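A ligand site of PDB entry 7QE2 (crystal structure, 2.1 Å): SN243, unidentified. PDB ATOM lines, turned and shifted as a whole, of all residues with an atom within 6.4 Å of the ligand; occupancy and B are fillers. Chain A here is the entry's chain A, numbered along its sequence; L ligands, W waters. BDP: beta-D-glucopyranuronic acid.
NE2 of His 303 lies within hydrogen-bond range of O1 of the ligand.
OD2 of Asp 385 lies within hydrogen-bond range of O2 of the ligand.
An oxygen (O6A) of the ligand sits at hydrogen-bond distance from the side-chain amide nitrogen (ND2) of Asn 156.
O6B of the ligand lies within hydrogen-bond range of OG1 of Thr 386 (2.7 Å).
O3 of the ligand sits at hydrogen-bond distance from NE2 of His 289, 2.8 Å away.
NH2 of Arg 106 is in salt-bridge range of O6B of the ligand (2.8 Å).
O3 of the ligand sits at hydrogen-bond distance from NH2 of Arg 242 (2.9 Å).
The side-chain amino group of Lys 288 sits at hydrogen-bond distance from an oxygen (O3) of the ligand, 3.1 Å away.
The side-chain hydroxyl (OH) of Tyr 339 is in hydrogen-bond range of an oxygen (O1) of the ligand (3.2 Å).
Tyr 228 touches the ligand.
CE1 of Tyr 338 touches O2 of the ligand, 3.9 Å away.
The nearest printed residue that does not touch the ligand is Met 336 (4.2 Å).
O of His 303 sits at hydrogen-bond distance from NE of Arg 392 (2.9 Å).
The backbone carbonyl oxygen of Thr 386 is in hydrogen-bond range of the side-chain hydroxyl of Tyr 339.
The backbone carbonyl oxygen (O) of Thr 386 sits at hydrogen-bond distance from the guanidinium group (NH1) of Arg 392 (3.3 Å).
NE of Arg 106 sits at hydrogen-bond distance from OG1 of Thr 72 (2.9 Å).
NH1 of Arg 242 is in hydrogen-bond range of OH of Tyr 338.
The side-chain amino group of Lys 288 is in hydrogen-bond range of the backbone carbonyl oxygen of Tyr 228, at 2.7 Å.
The side-chain hydroxyl (OH) of Tyr 228 lies within hydrogen-bond range of the side-chain hydroxyl (OG) of Ser 417.
O of Ser 155 sits at hydrogen-bond distance from N of Tyr 228.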
ATOM      1  N   THR A  72      24.639 -26.562  29.603  1.00  0.00           N
ATOM      2  CA  THR A  72      24.671 -26.317  31.034  1.00  0.00           C
ATOM      3  C   THR A  72      24.296 -27.561  31.822  1.00  0.00           C
ATOM      4  O   THR A  72      23.280 -28.203  31.548  1.00  0.00           O
ATOM      5  CB  THR A  72      23.706 -25.185  31.392  1.00  0.00           C
ATOM      6  OG1 THR A  72      24.013 -24.019  30.618  1.00  0.00           O
ATOM      7  CG2 THR A  72      23.762 -24.887  32.900  1.00  0.00           C
ATOM      8  N   VAL A 104      28.774 -27.214  30.902  1.00  0.00           N
ATOM      9  CA  VAL A 104      29.091 -25.893  31.446  1.00  0.00           C
ATOM     10  C   VAL A 104      28.579 -25.852  32.883  1.00  0.00           C
ATOM     11  O   VAL A 104      27.378 -26.069  33.124  1.00  0.00           O
ATOM     12  CB  VAL A 104      28.478 -24.776  30.593  1.00  0.00           C
ATOM     13  CG1 VAL A 104      28.972 -23.408  31.050  1.00  0.00           C
ATOM     14  CG2 VAL A 104      28.804 -25.013  29.125  1.00  0.00           C
ATOM     15  N   ARG A 106      27.855 -23.726  36.101  1.00  0.00           N
ATOM     16  CA  ARG A 106      27.613 -22.310  36.335  1.00  0.00           C
ATOM     17  C   ARG A 106      27.296 -21.948  37.782  1.00  0.00           C
ATOM     18  O   ARG A 106      27.000 -20.784  38.033  1.00  0.00           O
ATOM     19  CB  ARG A 106      26.480 -21.791  35.433  1.00  0.00           C
ATOM     20  CG  ARG A 106      26.542 -22.271  33.975  1.00  0.00           C
ATOM     21  CD  ARG A 106      25.605 -21.469  33.101  1.00  0.00           C
ATOM     22  NE  ARG A 106      25.614 -21.882  31.694  1.00  0.00           N
ATOM     23  CZ  ARG A 106      26.304 -21.260  30.739  1.00  0.00           C
ATOM     24  NH1 ARG A 106      27.038 -20.185  31.008  1.00  0.00           N
ATOM     25  NH2 ARG A 106      26.238 -21.699  29.498  1.00  0.00           N
ATOM     26  N   SER A 155      33.622 -23.490  32.213  1.00  0.00           N
ATOM     27  CA  SER A 155      32.981 -22.433  33.001  1.00  0.00           C
ATOM     28  C   SER A 155      33.535 -21.098  32.565  1.00  0.00           C
ATOM     29  O   SER A 155      34.658 -21.012  32.051  1.00  0.00           O
ATOM     30  CB  SER A 155      33.179 -22.641  34.512  1.00  0.00           C
ATOM     31  OG  SER A 155      33.087 -21.433  35.263  1.00  0.00           O
ATOM     32  N   ASN A 156      32.731 -20.054  32.750  1.00  0.00           N
ATOM     33  CA  ASN A 156      33.220 -18.690  32.644  1.00  0.00           C
ATOM     34  C   ASN A 156      34.093 -18.375  33.860  1.00  0.00           C
ATOM     35  O   ASN A 156      34.221 -19.157  34.785  1.00  0.00           O
ATOM     36  CB  ASN A 156      32.057 -17.717  32.525  1.00  0.00           C
ATOM     37  CG  ASN A 156      31.267 -17.927  31.255  1.00  0.00           C
ATOM     38  OD1 ASN A 156      31.804 -17.884  30.147  1.00  0.00           O
ATOM     39  ND2 ASN A 156      29.970 -18.160  31.410  1.00  0.00           N
ATOM     40  N   TYR A 228      35.387 -21.518  29.238  1.00  0.00           N
ATOM     41  CA  TYR A 228      34.862 -20.629  28.210  1.00  0.00           C
ATOM     42  C   TYR A 228      35.574 -19.291  28.406  1.00  0.00           C
ATOM     43  O   TYR A 228      35.088 -18.366  29.084  1.00  0.00           O
ATOM     44  CB  TYR A 228      33.341 -20.480  28.338  1.00  0.00           C
ATOM     45  CG  TYR A 228      32.485 -21.464  27.575  1.00  0.00           C
ATOM     46  CD1 TYR A 228      33.026 -22.460  26.750  1.00  0.00           C
ATOM     47  CD2 TYR A 228      31.082 -21.412  27.687  1.00  0.00           C
ATOM     48  CE1 TYR A 228      32.182 -23.345  26.020  1.00  0.00           C
ATOM     49  CE2 TYR A 228      30.263 -22.278  26.998  1.00  0.00           C
ATOM     50  CZ  TYR A 228      30.811 -23.241  26.159  1.00  0.00           C
ATOM     51  OH  TYR A 228      29.939 -24.085  25.479  1.00  0.00           O
ATOM     52  N   GLY A 229      36.760 -19.188  27.809  1.00  0.00           N
ATOM     53  CA  GLY A 229      37.633 -18.037  27.972  1.00  0.00           C
ATOM     54  C   GLY A 229      39.083 -18.449  27.979  1.00  0.00           C
ATOM     55  O   GLY A 229      39.419 -19.608  27.717  1.00  0.00           O
ATOM     56  N   MET A 231      38.922 -14.115  27.429  1.00  0.00           N
ATOM     57  CA  MET A 231      38.594 -13.267  26.297  1.00  0.00           C
ATOM     58  C   MET A 231      39.852 -12.575  25.780  1.00  0.00           C
ATOM     59  O   MET A 231      40.532 -11.857  26.540  1.00  0.00           O
ATOM     60  CB  MET A 231      37.547 -12.227  26.690  1.00  0.00           C
ATOM     61  CG  MET A 231      36.174 -12.798  26.723  1.00  0.00           C
ATOM     62  SD  MET A 231      34.936 -11.658  27.345  1.00  0.00           S
ATOM     63  CE  MET A 231      35.103 -10.339  26.148  1.00  0.00           C
ATOM     64  N   TYR A 241      29.461  -3.060  25.664  1.00  0.00           N
ATOM     65  CA  TYR A 241      29.283  -3.291  27.096  1.00  0.00           C
ATOM     66  C   TYR A 241      30.265  -4.329  27.640  1.00  0.00           C
ATOM     67  O   TYR A 241      30.560  -4.299  28.840  1.00  0.00           O
ATOM     68  CB  TYR A 241      27.827  -3.711  27.393  1.00  0.00           C
ATOM     69  CG  TYR A 241      27.472  -5.181  27.148  1.00  0.00           C
ATOM     70  CD1 TYR A 241      27.777  -6.173  28.089  1.00  0.00           C
ATOM     71  CD2 TYR A 241      26.819  -5.571  25.996  1.00  0.00           C
ATOM     72  CE1 TYR A 241      27.459  -7.525  27.864  1.00  0.00           C
ATOM     73  CE2 TYR A 241      26.512  -6.946  25.750  1.00  0.00           C
ATOM     74  CZ  TYR A 241      26.821  -7.893  26.696  1.00  0.00           C
ATOM     75  OH  TYR A 241      26.495  -9.220  26.455  1.00  0.00           O
ATOM     76  N   ARG A 242      30.804  -5.227  26.797  1.00  0.00           N
ATOM     77  CA  ARG A 242      31.709  -6.263  27.279  1.00  0.00           C
ATOM     78  C   ARG A 242      33.146  -5.781  27.432  1.00  0.00           C
ATOM     79  O   ARG A 242      34.013  -6.618  27.708  1.00  0.00           O
ATOM     80  CB  ARG A 242      31.681  -7.467  26.346  1.00  0.00           C
ATOM     81  CG  ARG A 242      30.269  -8.024  26.174  1.00  0.00           C
ATOM     82  CD  ARG A 242      30.248  -9.411  25.600  1.00  0.00           C
ATOM     83  NE  ARG A 242      30.605 -10.436  26.580  1.00  0.00           N
ATOM     84  CZ  ARG A 242      30.572 -11.734  26.316  1.00  0.00           C
ATOM     85  NH1 ARG A 242      30.192 -12.122  25.110  1.00  0.00           N
ATOM     86  NH2 ARG A 242      30.899 -12.613  27.251  1.00  0.00           N
ATOM     87  N   GLU A 245      35.077  -7.108  30.581  1.00  0.00           N
ATOM     88  CA  GLU A 245      35.794  -8.374  30.751  1.00  0.00           C
ATOM     89  C   GLU A 245      36.962  -8.487  29.769  1.00  0.00           C
ATOM     90  O   GLU A 245      37.483  -9.587  29.556  1.00  0.00           O
ATOM     91  CB  GLU A 245      34.859  -9.582  30.606  1.00  0.00           C
ATOM     92  CG  GLU A 245      33.742  -9.424  29.586  1.00  0.00           C
ATOM     93  CD  GLU A 245      32.693 -10.562  29.563  1.00  0.00           C
ATOM     94  OE1 GLU A 245      32.972 -11.645  30.115  1.00  0.00           O
ATOM     95  OE2 GLU A 245      31.599 -10.377  28.968  1.00  0.00           O
ATOM     96  N   LYS A 288      38.094 -16.974  23.372  1.00  0.00           N
ATOM     97  CA  LYS A 288      36.930 -16.333  22.802  1.00  0.00           C
ATOM     98  C   LYS A 288      37.185 -14.846  22.655  1.00  0.00           C
ATOM     99  O   LYS A 288      38.084 -14.294  23.310  1.00  0.00           O
ATOM    100  CB  LYS A 288      35.697 -16.590  23.689  1.00  0.00           C
ATOM    101  CG  LYS A 288      35.735 -15.953  25.071  1.00  0.00           C
ATOM    102  CD  LYS A 288      34.557 -16.477  25.912  1.00  0.00           C
ATOM    103  CE  LYS A 288      34.371 -15.702  27.213  1.00  0.00           C
ATOM    104  NZ  LYS A 288      33.460 -16.402  28.165  1.00  0.00           N
ATOM    105  N   HIS A 289      36.427 -14.172  21.783  1.00  0.00           N
ATOM    106  CA  HIS A 289      35.559 -14.780  20.772  1.00  0.00           C
ATOM    107  C   HIS A 289      36.130 -14.511  19.359  1.00  0.00           C
ATOM    108  O   HIS A 289      36.097 -13.386  18.856  1.00  0.00           O
ATOM    109  CB  HIS A 289      34.129 -14.242  20.861  1.00  0.00           C
ATOM    110  CG  HIS A 289      33.578 -14.167  22.255  1.00  0.00           C
ATOM    111  ND1 HIS A 289      33.909 -13.158  23.131  1.00  0.00           N
ATOM    112  CD2 HIS A 289      32.687 -14.958  22.901  1.00  0.00           C
ATOM    113  CE1 HIS A 289      33.255 -13.334  24.267  1.00  0.00           C
ATOM    114  NE2 HIS A 289      32.514 -14.418  24.150  1.00  0.00           N
ATOM    115  N   HIS A 303      24.837 -10.417  20.650  1.00  0.00           N
ATOM    116  CA  HIS A 303      23.784 -11.166  21.343  1.00  0.00           C
ATOM    117  C   HIS A 303      22.414 -10.728  20.875  1.00  0.00           C
ATOM    118  O   HIS A 303      21.450 -11.487  21.019  1.00  0.00           O
ATOM    119  CB  HIS A 303      23.834 -10.935  22.859  1.00  0.00           C
ATOM    120  CG  HIS A 303      24.830 -11.768  23.615  1.00  0.00           C
ATOM    121  ND1 HIS A 303      26.158 -11.423  23.715  1.00  0.00           N
ATOM    122  CD2 HIS A 303      24.665 -12.889  24.360  1.00  0.00           C
ATOM    123  CE1 HIS A 303      26.780 -12.334  24.452  1.00  0.00           C
ATOM    124  NE2 HIS A 303      25.890 -13.233  24.851  1.00  0.00           N
ATOM    125  N   MET A 336      36.421 -20.383  20.325  1.00  0.00           N
ATOM    126  CA  MET A 336      35.008 -20.059  20.229  1.00  0.00           C
ATOM    127  C   MET A 336      34.796 -18.839  19.321  1.00  0.00           C
ATOM    128  O   MET A 336      35.243 -17.728  19.660  1.00  0.00           O
ATOM    129  CB  MET A 336      34.427 -19.795  21.620  1.00  0.00           C
ATOM    130  CG  MET A 336      32.934 -19.412  21.607  1.00  0.00           C
ATOM    131  SD  MET A 336      32.297 -18.737  23.205  1.00  0.00           S
ATOM    132  CE  MET A 336      31.989 -20.256  24.112  1.00  0.00           C
ATOM    133  N   TYR A 338      32.693 -15.724  17.605  1.00  0.00           N
ATOM    134  CA  TYR A 338      31.644 -14.866  18.149  1.00  0.00           C
ATOM    135  C   TYR A 338      30.403 -14.902  17.261  1.00  0.00           C
ATOM    136  O   TYR A 338      30.429 -15.383  16.119  1.00  0.00           O
ATOM    137  CB  TYR A 338      32.108 -13.414  18.302  1.00  0.00           C
ATOM    138  CG  TYR A 338      31.324 -12.665  19.366  1.00  0.00           C
ATOM    139  CD1 TYR A 338      30.675 -13.358  20.381  1.00  0.00           C
ATOM    140  CD2 TYR A 338      31.224 -11.275  19.362  1.00  0.00           C
ATOM    141  CE1 TYR A 338      29.963 -12.702  21.376  1.00  0.00           C
ATOM    142  CE2 TYR A 338      30.519 -10.597  20.361  1.00  0.00           C
ATOM    143  CZ  TYR A 338      29.876 -11.326  21.356  1.00  0.00           C
ATOM    144  OH  TYR A 338      29.153 -10.704  22.348  1.00  0.00           O
ATOM    145  N   TYR A 339      29.313 -14.343  17.799  1.00  0.00           N
ATOM    146  CA  TYR A 339      28.059 -14.230  17.083  1.00  0.00           C
ATOM    147  C   TYR A 339      28.146 -13.269  15.897  1.00  0.00           C
ATOM    148  O   TYR A 339      27.347 -13.387  14.967  1.00  0.00           O
ATOM    149  CB  TYR A 339      26.956 -13.697  18.003  1.00  0.00           C
ATOM    150  CG  TYR A 339      26.723 -14.455  19.284  1.00  0.00           C
ATOM    151  CD1 TYR A 339      26.311 -15.790  19.254  1.00  0.00           C
ATOM    152  CD2 TYR A 339      26.848 -13.825  20.526  1.00  0.00           C
ATOM    153  CE1 TYR A 339      26.037 -16.475  20.420  1.00  0.00           C
ATOM    154  CE2 TYR A 339      26.589 -14.500  21.694  1.00  0.00           C
ATOM    155  CZ  TYR A 339      26.190 -15.820  21.642  1.00  0.00           C
ATOM    156  OH  TYR A 339      25.930 -16.496  22.810  1.00  0.00           O
ATOM    157  N   ASP A 385      29.630 -20.362  20.193  1.00  0.00           N
ATOM    158  CA  ASP A 385      29.063 -19.665  21.320  1.00  0.00           C
ATOM    159  C   ASP A 385      27.620 -20.126  21.517  1.00  0.00           C
ATOM    160  O   ASP A 385      26.999 -20.743  20.644  1.00  0.00           O
ATOM    161  CB  ASP A 385      29.128 -18.141  21.143  1.00  0.00           C
ATOM    162  CG  ASP A 385      29.187 -17.386  22.494  1.00  0.00           C
ATOM    163  OD1 ASP A 385      28.774 -17.927  23.543  1.00  0.00           O
ATOM    164  OD2 ASP A 385      29.654 -16.224  22.485  1.00  0.00           O
ATOM    165  N   THR A 386      27.074 -19.818  22.687  1.00  0.00           N
ATOM    166  CA  THR A 386      25.858 -20.466  23.138  1.00  0.00           C
ATOM    167  C   THR A 386      24.627 -19.910  22.401  1.00  0.00           C
ATOM    168  O   THR A 386      24.425 -18.685  22.331  1.00  0.00           O
ATOM    169  CB  THR A 386      25.740 -20.266  24.648  1.00  0.00           C
ATOM    170  OG1 THR A 386      26.912 -20.812  25.257  1.00  0.00           O
ATOM    171  CG2 THR A 386      24.497 -20.949  25.220  1.00  0.00           C
ATOM    172  N   ARG A 392      20.694 -17.080  17.558  1.00  0.00           N
ATOM    173  CA  ARG A 392      21.596 -16.088  16.956  1.00  0.00           C
ATOM    174  C   ARG A 392      22.227 -16.622  15.678  1.00  0.00           C
ATOM    175  O   ARG A 392      23.432 -16.527  15.454  1.00  0.00           O
ATOM    176  CB  ARG A 392      22.654 -15.649  17.992  1.00  0.00           C
ATOM    177  CG  ARG A 392      21.980 -14.953  19.186  1.00  0.00           C
ATOM    178  CD  ARG A 392      22.858 -14.700  20.418  1.00  0.00           C
ATOM    179  NE  ARG A 392      21.947 -14.336  21.500  1.00  0.00           N
ATOM    180  CZ  ARG A 392      21.508 -15.191  22.408  1.00  0.00           C
ATOM    181  NH1 ARG A 392      21.954 -16.441  22.414  1.00  0.00           N
ATOM    182  NH2 ARG A 392      20.624 -14.790  23.314  1.00  0.00           N
ATOM    183  N   SER A 417      27.346 -25.169  21.525  1.00  0.00           N
ATOM    184  CA  SER A 417      26.939 -24.782  22.878  1.00  0.00           C
ATOM    185  C   SER A 417      25.455 -24.428  22.905  1.00  0.00           C
ATOM    186  O   SER A 417      24.981 -23.618  22.102  1.00  0.00           O
ATOM    187  CB  SER A 417      27.766 -23.596  23.361  1.00  0.00           C
ATOM    188  OG  SER A 417      27.511 -23.344  24.748  1.00  0.00           O
ATOM    189  N   PHE A 622      21.594  -9.695  28.690  1.00  0.00           N
ATOM    190  CA  PHE A 622      23.022  -9.936  28.823  1.00  0.00           C
ATOM    191  C   PHE A 622      23.816  -8.693  29.213  1.00  0.00           C
ATOM    192  O   PHE A 622      25.000  -8.819  29.524  1.00  0.00           O
ATOM    193  CB  PHE A 622      23.583 -10.510  27.541  1.00  0.00           C
ATOM    194  CG  PHE A 622      22.852 -11.735  27.068  1.00  0.00           C
ATOM    195  CD1 PHE A 622      23.285 -13.010  27.457  1.00  0.00           C
ATOM    196  CD2 PHE A 622      21.744 -11.619  26.243  1.00  0.00           C
ATOM    197  CE1 PHE A 622      22.621 -14.134  27.024  1.00  0.00           C
ATOM    198  CE2 PHE A 622      21.065 -12.769  25.797  1.00  0.00           C
ATOM    199  CZ  PHE A 622      21.512 -14.026  26.193  1.00  0.00           C
HETATM  200  C1  BDP L   1      27.538 -16.330  25.785  1.00  0.00           C
HETATM  201  C2  BDP L   1      28.815 -15.486  25.761  1.00  0.00           C
HETATM  202  C3  BDP L   1      30.086 -16.276  26.096  1.00  0.00           C
HETATM  203  C4  BDP L   1      29.828 -17.231  27.258  1.00  0.00           C
HETATM  204  C5  BDP L   1      28.581 -18.074  26.949  1.00  0.00           C
HETATM  205  C6  BDP L   1      28.283 -19.067  28.033  1.00  0.00           C
HETATM  206  O2  BDP L   1      28.949 -14.805  24.515  1.00  0.00           O
HETATM  207  O3  BDP L   1      31.161 -15.381  26.370  1.00  0.00           O
HETATM  208  O4  BDP L   1      30.944 -18.081  27.523  1.00  0.00           O
HETATM  209  O5  BDP L   1      27.466 -17.189  26.912  1.00  0.00           O
HETATM  210  O6A BDP L   1      28.679 -18.873  29.162  1.00  0.00           O
HETATM  211  O1  BDP L   1      26.442 -15.519  25.833  1.00  0.00           O
HETATM  212  O6B BDP L   1      27.692 -20.089  27.741  1.00  0.00           O
HETATM  213  O   HOH W   1      23.756 -16.974  25.569  1.00  0.00           O
HETATM  214  O   HOH W   2      27.029 -13.729  28.760  1.00  0.00           O
